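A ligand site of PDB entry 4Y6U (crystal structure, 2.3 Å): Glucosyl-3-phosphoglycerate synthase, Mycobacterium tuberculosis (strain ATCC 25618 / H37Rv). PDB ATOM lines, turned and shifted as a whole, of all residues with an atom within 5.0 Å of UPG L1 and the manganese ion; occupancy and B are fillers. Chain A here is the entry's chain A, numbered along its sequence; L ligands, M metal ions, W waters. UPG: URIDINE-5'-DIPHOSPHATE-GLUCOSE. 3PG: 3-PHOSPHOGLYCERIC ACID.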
ATOM      1  N   PRO A  54      11.958 -11.886  12.902  1.00  0.00           N
ATOM      2  CA  PRO A  54      12.577 -13.050  12.266  1.00  0.00           C
ATOM      3  C   PRO A  54      13.957 -12.673  11.784  1.00  0.00           C
ATOM      4  O   PRO A  54      14.154 -11.580  11.235  1.00  0.00           O
ATOM      5  CB  PRO A  54      11.646 -13.338  11.095  1.00  0.00           C
ATOM      6  CG  PRO A  54      11.162 -12.023  10.718  1.00  0.00           C
ATOM      7  CD  PRO A  54      11.050 -11.206  11.977  1.00  0.00           C
ATOM      8  N   ALA A  55      14.889 -13.601  11.898  1.00  0.00           N
ATOM      9  CA  ALA A  55      16.274 -13.290  11.559  1.00  0.00           C
ATOM     10  C   ALA A  55      16.996 -14.511  11.017  1.00  0.00           C
ATOM     11  O   ALA A  55      17.072 -15.555  11.676  1.00  0.00           O
ATOM     12  CB  ALA A  55      16.997 -12.726  12.781  1.00  0.00           C
ATOM     13  N   LEU A  56      17.512 -14.367   9.796  1.00  0.00           N
ATOM     14  CA  LEU A  56      18.452 -15.318   9.217  1.00  0.00           C
ATOM     15  C   LEU A  56      19.716 -14.559   8.832  1.00  0.00           C
ATOM     16  O   LEU A  56      19.729 -13.864   7.828  1.00  0.00           O
ATOM     17  CB  LEU A  56      17.862 -16.011   7.986  1.00  0.00           C
ATOM     18  CG  LEU A  56      18.767 -16.876   7.112  1.00  0.00           C
ATOM     19  CD1 LEU A  56      19.314 -18.018   7.937  1.00  0.00           C
ATOM     20  CD2 LEU A  56      18.003 -17.449   5.870  1.00  0.00           C
ATOM     21  N   GLU A  58      21.612 -11.908  10.211  1.00  0.00           N
ATOM     22  CA  GLU A  58      21.441 -10.466  10.162  1.00  0.00           C
ATOM     23  C   GLU A  58      22.299  -9.770  11.236  1.00  0.00           C
ATOM     24  O   GLU A  58      21.882  -8.752  11.802  1.00  0.00           O
ATOM     25  CB  GLU A  58      19.964 -10.095  10.361  1.00  0.00           C
ATOM     26  CG  GLU A  58      18.997 -10.666   9.336  1.00  0.00           C
ATOM     27  CD  GLU A  58      19.239 -10.210   7.896  1.00  0.00           C
ATOM     28  OE1 GLU A  58      20.140  -9.378   7.604  1.00  0.00           O
ATOM     29  OE2 GLU A  58      18.513 -10.692   7.005  1.00  0.00           O
ATOM     30  N   LEU A  83      13.101 -14.356  16.453  1.00  0.00           N
ATOM     31  CA  LEU A  83      12.911 -15.751  15.964  1.00  0.00           C
ATOM     32  C   LEU A  83      14.078 -16.059  15.025  1.00  0.00           C
ATOM     33  O   LEU A  83      14.073 -15.639  13.873  1.00  0.00           O
ATOM     34  CB  LEU A  83      11.552 -15.941  15.244  1.00  0.00           C
ATOM     35  CG  LEU A  83      11.005 -17.370  15.106  1.00  0.00           C
ATOM     36  CD1 LEU A  83      11.983 -18.380  14.475  1.00  0.00           C
ATOM     37  CD2 LEU A  83      10.549 -17.893  16.456  1.00  0.00           C
ATOM     38  N   SER A  85      16.129 -18.012  12.578  1.00  0.00           N
ATOM     39  CA  SER A  85      15.761 -18.941  11.524  1.00  0.00           C
ATOM     40  C   SER A  85      16.940 -19.750  10.993  1.00  0.00           C
ATOM     41  O   SER A  85      17.053 -19.960   9.786  1.00  0.00           O
ATOM     42  CB  SER A  85      15.128 -18.170  10.371  1.00  0.00           C
ATOM     43  OG  SER A  85      14.386 -19.034   9.536  1.00  0.00           O
ATOM     44  N   GLY A 117      12.583 -21.422   5.421  1.00  0.00           N
ATOM     45  CA  GLY A 117      11.883 -20.324   4.775  1.00  0.00           C
ATOM     46  C   GLY A 117      11.325 -19.367   5.802  1.00  0.00           C
ATOM     47  O   GLY A 117      11.101 -19.758   6.936  1.00  0.00           O
ATOM     48  N   LYS A 118      11.082 -18.123   5.414  1.00  0.00           N
ATOM     49  CA  LYS A 118      10.477 -17.146   6.317  1.00  0.00           C
ATOM     50  C   LYS A 118       9.081 -17.515   6.878  1.00  0.00           C
ATOM     51  O   LYS A 118       8.843 -17.369   8.074  1.00  0.00           O
ATOM     52  CB  LYS A 118      10.396 -15.795   5.613  1.00  0.00           C
ATOM     53  CG  LYS A 118      10.198 -14.635   6.572  1.00  0.00           C
ATOM     54  CD  LYS A 118       9.787 -13.375   5.846  1.00  0.00           C
ATOM     55  CE  LYS A 118       9.611 -12.200   6.841  1.00  0.00           C
ATOM     56  NZ  LYS A 118       8.962 -10.967   6.286  1.00  0.00           N
ATOM     57  N   ALA A 121       9.100 -19.578   9.914  1.00  0.00           N
ATOM     58  CA  ALA A 121       9.616 -18.856  11.086  1.00  0.00           C
ATOM     59  C   ALA A 121       8.517 -18.005  11.716  1.00  0.00           C
ATOM     60  O   ALA A 121       8.321 -18.007  12.945  1.00  0.00           O
ATOM     61  CB  ALA A 121      10.808 -18.013  10.685  1.00  0.00           C
ATOM     62  N   ASP A 138      11.039  -6.716  10.114  1.00  0.00           N
ATOM     63  CA  ASP A 138      12.257  -7.332   9.553  1.00  0.00           C
ATOM     64  C   ASP A 138      13.521  -6.843  10.288  1.00  0.00           C
ATOM     65  O   ASP A 138      13.630  -5.711  10.768  1.00  0.00           O
ATOM     66  CB  ASP A 138      12.373  -7.050   8.050  1.00  0.00           C
ATOM     67  CG  ASP A 138      11.404  -7.938   7.187  1.00  0.00           C
ATOM     68  OD1 ASP A 138      10.790  -8.868   7.731  1.00  0.00           O
ATOM     69  OD2 ASP A 138      11.310  -7.724   5.958  1.00  0.00           O
ATOM     70  N   SER A 139      14.511  -7.715  10.322  1.00  0.00           N
ATOM     71  CA  SER A 139      15.677  -7.520  11.155  1.00  0.00           C
ATOM     72  C   SER A 139      16.919  -7.049  10.348  1.00  0.00           C
ATOM     73  O   SER A 139      18.014  -6.943  10.894  1.00  0.00           O
ATOM     74  CB  SER A 139      15.951  -8.817  11.893  1.00  0.00           C
ATOM     75  OG  SER A 139      16.323  -9.791  10.943  1.00  0.00           O
ATOM     76  N   ASP A 140      16.706  -6.778   9.051  1.00  0.00           N
ATOM     77  CA  ASP A 140      17.746  -6.349   8.132  1.00  0.00           C
ATOM     78  C   ASP A 140      17.578  -4.863   7.809  1.00  0.00           C
ATOM     79  O   ASP A 140      18.244  -4.350   6.903  1.00  0.00           O
ATOM     80  CB  ASP A 140      17.703  -7.146   6.803  1.00  0.00           C
ATOM     81  CG  ASP A 140      16.497  -6.804   5.950  1.00  0.00           C
ATOM     82  OD1 ASP A 140      15.414  -6.547   6.530  1.00  0.00           O
ATOM     83  OD2 ASP A 140      16.608  -6.781   4.692  1.00  0.00           O
ATOM     84  N   LEU A 213       3.830  -6.719  -0.027  1.00  0.00           N
ATOM     85  CA  LEU A 213       4.909  -7.574   0.464  1.00  0.00           C
ATOM     86  C   LEU A 213       5.656  -7.028   1.697  1.00  0.00           C
ATOM     87  O   LEU A 213       6.663  -7.581   2.113  1.00  0.00           O
ATOM     88  CB  LEU A 213       5.917  -7.799  -0.665  1.00  0.00           C
ATOM     89  CG  LEU A 213       5.335  -8.424  -1.962  1.00  0.00           C
ATOM     90  CD1 LEU A 213       6.435  -8.875  -2.921  1.00  0.00           C
ATOM     91  CD2 LEU A 213       4.428  -9.597  -1.621  1.00  0.00           C
ATOM     92  N   SER A 214       5.184  -5.956   2.300  1.00  0.00           N
ATOM     93  CA  SER A 214       5.959  -5.368   3.373  1.00  0.00           C
ATOM     94  C   SER A 214       6.140  -6.324   4.541  1.00  0.00           C
ATOM     95  O   SER A 214       5.197  -6.974   5.005  1.00  0.00           O
ATOM     96  CB  SER A 214       5.328  -4.092   3.865  1.00  0.00           C
ATOM     97  OG  SER A 214       6.185  -3.511   4.814  1.00  0.00           O
ATOM     98  N   GLY A 215       7.367  -6.360   5.049  1.00  0.00           N
ATOM     99  CA  GLY A 215       7.707  -7.217   6.167  1.00  0.00           C
ATOM    100  C   GLY A 215       7.315  -6.629   7.512  1.00  0.00           C
ATOM    101  O   GLY A 215       7.393  -7.316   8.541  1.00  0.00           O
ATOM    102  N   TYR A 233       9.089 -17.091   1.141  1.00  0.00           N
ATOM    103  CA  TYR A 233       8.640 -15.711   0.899  1.00  0.00           C
ATOM    104  C   TYR A 233       7.167 -15.532   0.429  1.00  0.00           C
ATOM    105  O   TYR A 233       6.719 -14.417   0.127  1.00  0.00           O
ATOM    106  CB  TYR A 233       9.577 -15.084  -0.145  1.00  0.00           C
ATOM    107  CG  TYR A 233      10.947 -14.828   0.404  1.00  0.00           C
ATOM    108  CD1 TYR A 233      11.135 -13.962   1.473  1.00  0.00           C
ATOM    109  CD2 TYR A 233      12.055 -15.473  -0.108  1.00  0.00           C
ATOM    110  CE1 TYR A 233      12.372 -13.741   2.003  1.00  0.00           C
ATOM    111  CE2 TYR A 233      13.294 -15.270   0.405  1.00  0.00           C
ATOM    112  CZ  TYR A 233      13.464 -14.390   1.445  1.00  0.00           C
ATOM    113  OH  TYR A 233      14.762 -14.195   1.934  1.00  0.00           O
ATOM    114  N   VAL A 235       4.654 -16.016   2.372  1.00  0.00           N
ATOM    115  CA  VAL A 235       3.807 -15.761   3.530  1.00  0.00           C
ATOM    116  C   VAL A 235       3.060 -14.419   3.497  1.00  0.00           C
ATOM    117  O   VAL A 235       1.856 -14.404   3.776  1.00  0.00           O
ATOM    118  CB  VAL A 235       4.649 -15.911   4.865  1.00  0.00           C
ATOM    119  CG1 VAL A 235       5.824 -14.940   4.930  1.00  0.00           C
ATOM    120  CG2 VAL A 235       3.733 -15.837   6.127  1.00  0.00           C
ATOM    121  N   GLU A 236       3.695 -13.296   3.142  1.00  0.00           N
ATOM    122  CA  GLU A 236       2.961 -12.020   3.180  1.00  0.00           C
ATOM    123  C   GLU A 236       1.791 -11.976   2.189  1.00  0.00           C
ATOM    124  O   GLU A 236       0.678 -11.547   2.522  1.00  0.00           O
ATOM    125  CB  GLU A 236       3.832 -10.819   2.876  1.00  0.00           C
ATOM    126  CG  GLU A 236       4.702 -10.321   4.006  1.00  0.00           C
ATOM    127  CD  GLU A 236       5.837 -11.254   4.307  1.00  0.00           C
ATOM    128  OE1 GLU A 236       6.164 -11.388   5.501  1.00  0.00           O
ATOM    129  OE2 GLU A 236       6.396 -11.870   3.366  1.00  0.00           O
ATOM    130  N   ILE A 237       2.039 -12.370   0.963  1.00  0.00           N
ATOM    131  CA  ILE A 237       0.990 -12.251  -0.042  1.00  0.00           C
ATOM    132  C   ILE A 237      -0.170 -13.224   0.269  1.00  0.00           C
ATOM    133  O   ILE A 237      -1.328 -12.929  -0.029  1.00  0.00           O
ATOM    134  CB  ILE A 237       1.553 -12.476  -1.468  1.00  0.00           C
ATOM    135  CG1 ILE A 237       0.578 -11.955  -2.516  1.00  0.00           C
ATOM    136  CG2 ILE A 237       1.891 -13.956  -1.724  1.00  0.00           C
ATOM    137  CD1 ILE A 237       0.409 -10.464  -2.479  1.00  0.00           C
ATOM    138  N   ARG A 260      12.310   3.312   3.720  1.00  0.00           N
ATOM    139  CA  ARG A 260      12.743   1.968   4.077  1.00  0.00           C
ATOM    140  C   ARG A 260      14.050   1.643   3.395  1.00  0.00           C
ATOM    141  O   ARG A 260      14.208   1.847   2.197  1.00  0.00           O
ATOM    142  CB  ARG A 260      11.680   0.952   3.682  1.00  0.00           C
ATOM    143  CG  ARG A 260      11.668  -0.302   4.562  1.00  0.00           C
ATOM    144  CD  ARG A 260      11.355  -1.516   3.722  1.00  0.00           C
ATOM    145  NE  ARG A 260      10.895  -2.650   4.512  1.00  0.00           N
ATOM    146  CZ  ARG A 260      11.031  -3.913   4.120  1.00  0.00           C
ATOM    147  NH1 ARG A 260      10.574  -4.928   4.885  1.00  0.00           N
ATOM    148  NH2 ARG A 260      11.630  -4.150   2.951  1.00  0.00           N
ATOM    149  N   HIS A 262      17.091  -1.519   3.410  1.00  0.00           N
ATOM    150  CA  HIS A 262      17.313  -2.864   3.867  1.00  0.00           C
ATOM    151  C   HIS A 262      18.328  -3.516   2.958  1.00  0.00           C
ATOM    152  O   HIS A 262      18.933  -2.847   2.129  1.00  0.00           O
ATOM    153  CB  HIS A 262      15.988  -3.665   3.903  1.00  0.00           C
ATOM    154  CG  HIS A 262      15.409  -3.957   2.547  1.00  0.00           C
ATOM    155  ND1 HIS A 262      15.069  -5.229   2.137  1.00  0.00           N
ATOM    156  CD2 HIS A 262      15.088  -3.125   1.524  1.00  0.00           C
ATOM    157  CE1 HIS A 262      14.585  -5.178   0.905  1.00  0.00           C
ATOM    158  NE2 HIS A 262      14.574  -3.915   0.526  1.00  0.00           N
ATOM    159  N   ARG A 263      18.553  -4.816   3.141  1.00  0.00           N
ATOM    160  CA  ARG A 263      19.554  -5.524   2.368  1.00  0.00           C
ATOM    161  C   ARG A 263      19.115  -5.582   0.917  1.00  0.00           C
ATOM    162  O   ARG A 263      17.989  -5.964   0.623  1.00  0.00           O
ATOM    163  CB  ARG A 263      19.789  -6.926   2.946  1.00  0.00           C
ATOM    164  CG  ARG A 263      20.864  -7.744   2.218  1.00  0.00           C
ATOM    165  CD  ARG A 263      20.868  -9.211   2.638  1.00  0.00           C
ATOM    166  NE  ARG A 263      21.119  -9.388   4.075  1.00  0.00           N
ATOM    167  CZ  ARG A 263      22.300  -9.606   4.618  1.00  0.00           C
ATOM    168  NH1 ARG A 263      23.382  -9.677   3.871  1.00  0.00           N
ATOM    169  NH2 ARG A 263      22.407  -9.766   5.925  1.00  0.00           N
ATOM    170  N   ARG A 265      19.347  -7.388  -2.507  1.00  0.00           N
ATOM    171  CA  ARG A 265      19.718  -8.762  -2.840  1.00  0.00           C
ATOM    172  C   ARG A 265      19.971  -8.877  -4.326  1.00  0.00           C
ATOM    173  O   ARG A 265      19.416  -8.108  -5.115  1.00  0.00           O
ATOM    174  CB  ARG A 265      18.613  -9.734  -2.397  1.00  0.00           C
ATOM    175  CG  ARG A 265      18.461  -9.863  -0.895  1.00  0.00           C
ATOM    176  CD  ARG A 265      17.139 -10.516  -0.560  1.00  0.00           C
ATOM    177  NE  ARG A 265      17.174 -11.968  -0.750  1.00  0.00           N
ATOM    178  CZ  ARG A 265      16.107 -12.736  -0.966  1.00  0.00           C
ATOM    179  NH1 ARG A 265      14.878 -12.206  -1.069  1.00  0.00           N
ATOM    180  NH2 ARG A 265      16.259 -14.045  -1.121  1.00  0.00           N
ATOM    181  N   LEU A 270      16.065 -12.821  -6.056  1.00  0.00           N
ATOM    182  CA  LEU A 270      14.765 -12.195  -6.148  1.00  0.00           C
ATOM    183  C   LEU A 270      13.858 -12.984  -7.088  1.00  0.00           C
ATOM    184  O   LEU A 270      12.657 -12.990  -6.899  1.00  0.00           O
ATOM    185  CB  LEU A 270      14.897 -10.750  -6.630  1.00  0.00           C
ATOM    186  CG  LEU A 270      15.532  -9.743  -5.676  1.00  0.00           C
ATOM    187  CD1 LEU A 270      15.490  -8.390  -6.316  1.00  0.00           C
ATOM    188  CD2 LEU A 270      14.873  -9.698  -4.313  1.00  0.00           C
ATOM    189  N   MET A 273      12.453 -15.688  -5.182  1.00  0.00           N
ATOM    190  CA  MET A 273      11.445 -15.148  -4.280  1.00  0.00           C
ATOM    191  C   MET A 273      10.155 -14.916  -5.017  1.00  0.00           C
ATOM    192  O   MET A 273       9.077 -15.231  -4.536  1.00  0.00           O
ATOM    193  CB  MET A 273      11.902 -13.816  -3.669  1.00  0.00           C
ATOM    194  CG  MET A 273      10.809 -13.159  -2.869  1.00  0.00           C
ATOM    195  SD  MET A 273      11.315 -11.831  -1.754  1.00  0.00           S
ATOM    196  CE  MET A 273      11.737 -10.618  -2.975  1.00  0.00           C
ATOM    197  N   VAL A 277       6.295 -16.258  -4.550  1.00  0.00           N
ATOM    198  CA  VAL A 277       5.196 -15.293  -4.454  1.00  0.00           C
ATOM    199  C   VAL A 277       4.102 -15.640  -5.468  1.00  0.00           C
ATOM    200  O   VAL A 277       2.907 -15.513  -5.210  1.00  0.00           O
ATOM    201  CB  VAL A 277       5.688 -13.855  -4.705  1.00  0.00           C
ATOM    202  CG1 VAL A 277       4.550 -12.896  -4.842  1.00  0.00           C
ATOM    203  CG2 VAL A 277       6.563 -13.400  -3.564  1.00  0.00           C
HETATM  204  N1  UPG L   1      14.215 -14.355   6.993  1.00  0.00           N
HETATM  205  C2  UPG L   1      14.054 -15.439   7.879  1.00  0.00           C
HETATM  206  N3  UPG L   1      14.097 -16.712   7.398  1.00  0.00           N
HETATM  207  C4  UPG L   1      14.293 -16.949   6.082  1.00  0.00           C
HETATM  208  C5  UPG L   1      14.432 -15.884   5.183  1.00  0.00           C
HETATM  209  C6  UPG L   1      14.357 -14.584   5.659  1.00  0.00           C
HETATM  210  O2  UPG L   1      13.891 -15.210   9.089  1.00  0.00           O
HETATM  211  O4  UPG L   1      14.360 -18.130   5.663  1.00  0.00           O
HETATM  212  C1C UPG L   1      14.092 -12.991   7.484  1.00  0.00           C
HETATM  213  C2C UPG L   1      15.263 -12.089   7.106  1.00  0.00           C
HETATM  214  O2C UPG L   1      16.259 -12.251   8.095  1.00  0.00           O
HETATM  215  C3C UPG L   1      14.613 -10.732   7.109  1.00  0.00           C
HETATM  216  C4C UPG L   1      13.153 -11.000   6.738  1.00  0.00           C
HETATM  217  O4C UPG L   1      12.927 -12.395   6.907  1.00  0.00           O
HETATM  218  O3C UPG L   1      14.753 -10.185   8.412  1.00  0.00           O
HETATM  219  C5C UPG L   1      12.882 -10.573   5.295  1.00  0.00           C
HETATM  220  O5C UPG L   1      13.744 -11.355   4.477  1.00  0.00           O
HETATM  221  PA  UPG L   1      14.535 -10.714   3.239  1.00  0.00           P
HETATM  222  O1A UPG L   1      15.256  -9.426   3.680  1.00  0.00           O
HETATM  223  O2A UPG L   1      15.571 -11.743   2.842  1.00  0.00           O
HETATM  224  O3A UPG L   1      13.340 -10.435   2.179  1.00  0.00           O
HETATM  225  PB  UPG L   1      13.133  -9.208   1.126  1.00  0.00           P
HETATM  226  O1B UPG L   1      14.029  -9.425  -0.047  1.00  0.00           O
HETATM  227  O2B UPG L   1      13.216  -7.847   1.772  1.00  0.00           O
HETATM  228  O3B UPG L   1      11.613  -9.432   0.686  1.00  0.00           O
HETATM  229  C1' UPG L   1      10.494  -8.535   0.833  1.00  0.00           C
HETATM  230  C2' UPG L   1      10.128  -8.226   2.297  1.00  0.00           C
HETATM  231  C3' UPG L   1       9.995  -9.520   3.088  1.00  0.00           C
HETATM  232  C4' UPG L   1       8.938 -10.374   2.426  1.00  0.00           C
HETATM  233  C5' UPG L   1       9.204 -10.542   0.945  1.00  0.00           C
HETATM  234  C6' UPG L   1       8.063 -11.393   0.333  1.00  0.00           C
HETATM  235  O2' UPG L   1      11.089  -7.371   2.931  1.00  0.00           O
HETATM  236  O3' UPG L   1       9.696  -9.237   4.470  1.00  0.00           O
HETATM  237  O4' UPG L   1       8.846 -11.688   3.009  1.00  0.00           O
HETATM  238  O5' UPG L   1       9.378  -9.266   0.319  1.00  0.00           O
HETATM  239  O6' UPG L   1       6.820 -11.002   0.913  1.00  0.00           O
HETATM  240  C1  3PG L   2      10.482  -6.494  -2.611  1.00  0.00           C
HETATM  241  O1  3PG L   2       9.757  -7.069  -1.761  1.00  0.00           O
HETATM  242  O2  3PG L   2       9.876  -6.010  -3.609  1.00  0.00           O
HETATM  243  C2  3PG L   2      12.013  -6.382  -2.494  1.00  0.00           C
HETATM  244  O3  3PG L   2      12.567  -7.264  -1.542  1.00  0.00           O
HETATM  245  C3  3PG L   2      12.498  -4.988  -2.154  1.00  0.00           C
HETATM  246  O1P 3PG L   2      13.889  -4.883  -2.447  1.00  0.00           O
HETATM  247  P   3PG L   2      14.328  -3.879  -3.587  1.00  0.00           P
HETATM  248  O2P 3PG L   2      13.977  -4.432  -4.960  1.00  0.00           O
HETATM  249  O3P 3PG L   2      13.556  -2.625  -3.321  1.00  0.00           O
HETATM  250  O4P 3PG L   2      15.808  -3.544  -3.554  1.00  0.00           O
HETATM  251 MN    MN M   1      15.026  -7.252   3.151  1.00  0.00          MN
HETATM  252  O   HOH W   1      13.659  -6.578   4.729  1.00  0.00           O
HETATM  253  O   HOH W   2      16.554  -7.894   1.697  1.00  0.00           O
HETATM  254  O   HOH W   3       4.665 -12.854   0.023  1.00  0.00           O
HETATM  255  O   HOH W   4      15.159 -20.788   6.437  1.00  0.00           O
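OE2 of Glu 236 is in hydrogen-bond range of O4' of UPG L1. N of Lys 118 is in hydrogen-bond range of O4 of UPG L1 (3.3 Å). The side-chain amino group (NZ) of Lys 118 lies within hydrogen-bond range of an oxygen (O3') of UPG L1 (2.6 Å). The side-chain carboxylate (OD2) of Asp 138 lies within hydrogen-bond range of an oxygen (O3') of UPG L1, 2.7 Å away. The side-chain hydroxyl of Tyr 233 is in hydrogen-bond range of an oxygen (O2A) of UPG L1. The side-chain carboxylate (OE2) of Glu 58 lies within hydrogen-bond range of an oxygen (O2C) of UPG L1. An oxygen (O2C) of UPG L1 sits at hydrogen-bond distance from the backbone NH (N) of Leu 56. An oxygen (O3C) of UPG L1 lies within hydrogen-bond range of the backbone NH (N) of Ser 139. The side-chain hydroxyl of Ser 139 lies within hydrogen-bond range of an oxygen (O3C) of UPG L1 (3.0 Å). NH1 of Arg 265 is in salt-bridge range of O1B of UPG L1, at 3.1 Å. OG of Ser 85 sits at hydrogen-bond distance from N3 of UPG L1, 3.2 Å away. O2' of UPG L1 sits at hydrogen-bond distance from NH1 of Arg 260, at 3.2 Å. The backbone carbonyl oxygen (O) of Pro 54 sits at hydrogen-bond distance from an oxygen (O3C) of UPG L1, 3.2 Å away. The backbone NH of Ala 55 lies within hydrogen-bond range of an oxygen (O2) of UPG L1. NE2 of His 262 sits at hydrogen-bond distance from O1P of 3PG L2 (3.2 Å).
An oxygen (O1B) of UPG L1 lies within hydrogen-bond range of an oxygen (O3) of 3PG L2, 3.0 Å away.
The side-chain amino group of Lys 118 lies within salt-bridge range of the side-chain carboxylate of Glu 236 (2.9 Å). NZ of Lys 118 is in salt-bridge range of OD1 of Asp 138, 3.1 Å away. The side-chain carboxylate (OD2) of Asp 138 lies within salt-bridge range of the guanidinium group (NH1) of Arg 260, at 3.1 Å. The guanidinium group of Arg 265 is in hydrogen-bond range of the side-chain hydroxyl of Tyr 233 (3.4 Å). NH2 of Arg 263 is in salt-bridge range of OE1 of Glu 58. The side-chain hydroxyl (OG) of Ser 139 sits at hydrogen-bond distance from the backbone carbonyl oxygen (O) of Pro 54, 2.8 Å away. N of Ser 85 lies within hydrogen-bond range of O of Ala 55. The backbone NH (N) of Ala 55 lies within hydrogen-bond range of the backbone carbonyl oxygen (O) of Leu 83.
The side-chain sulfur of Met 273 lies close to an oxygen (O3B) of UPG L1 (3.4 Å). Gly 117 touches UPG L1 (C to O4, 3.3 Å). O of Leu 213 touches C2' of UPG L1, 3.5 Å away. Gly 215 touches UPG L1 (CA to O3', 3.3 Å). Hydrophobic or aromatic side chains that line UPG L1: Pro 54, Leu 56, Leu 213, Tyr 233, His 262 and Met 273. Within 4 Å of UPG L1: Pro 54, Ala 55, Leu 56, Glu 58, Ser 85, Gly 117, Lys 118, Asp 138, Ser 139, Asp 140, Leu 213, Gly 215, Tyr 233, Glu 236, Arg 260, His 262, Arg 265 and Met 273.
The nearest printed residue that does not touch the manganese ion is Arg 263 (4.1 Å).
The manganese ion is bound by water W1 (2.2 Å), water W2 (2.2 Å), O1A of UPG L1 (2.2 Å), OD2 of Asp 140 (2.3 Å), ND1 of His 262 (2.3 Å) and O2B of UPG L1 (2.4 Å). The manganese ion has six donor atoms within binding distance.
Water W2 lies within hydrogen-bond range of the backbone carbonyl oxygen (O) of Arg 263 (2.6 Å) and an oxygen (O1B) of UPG L1 (3.4 Å). Water W1 lies within hydrogen-bond range of OD1 of Asp 140 (2.5 Å), OD2 of Asp 138 (2.9 Å) and O2' of UPG L1 (3.2 Å). Water W4 lies within hydrogen-bond range of N of Gly 117 (2.8 Å) and O4 of UPG L1 (2.9 Å). Water W3 lies within hydrogen-bond range of the backbone carbonyl oxygen (O) of Tyr 233, the backbone NH (N) of Ile 237, an oxygen (O6') of UPG L1 and the backbone NH (N) of Glu 236.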
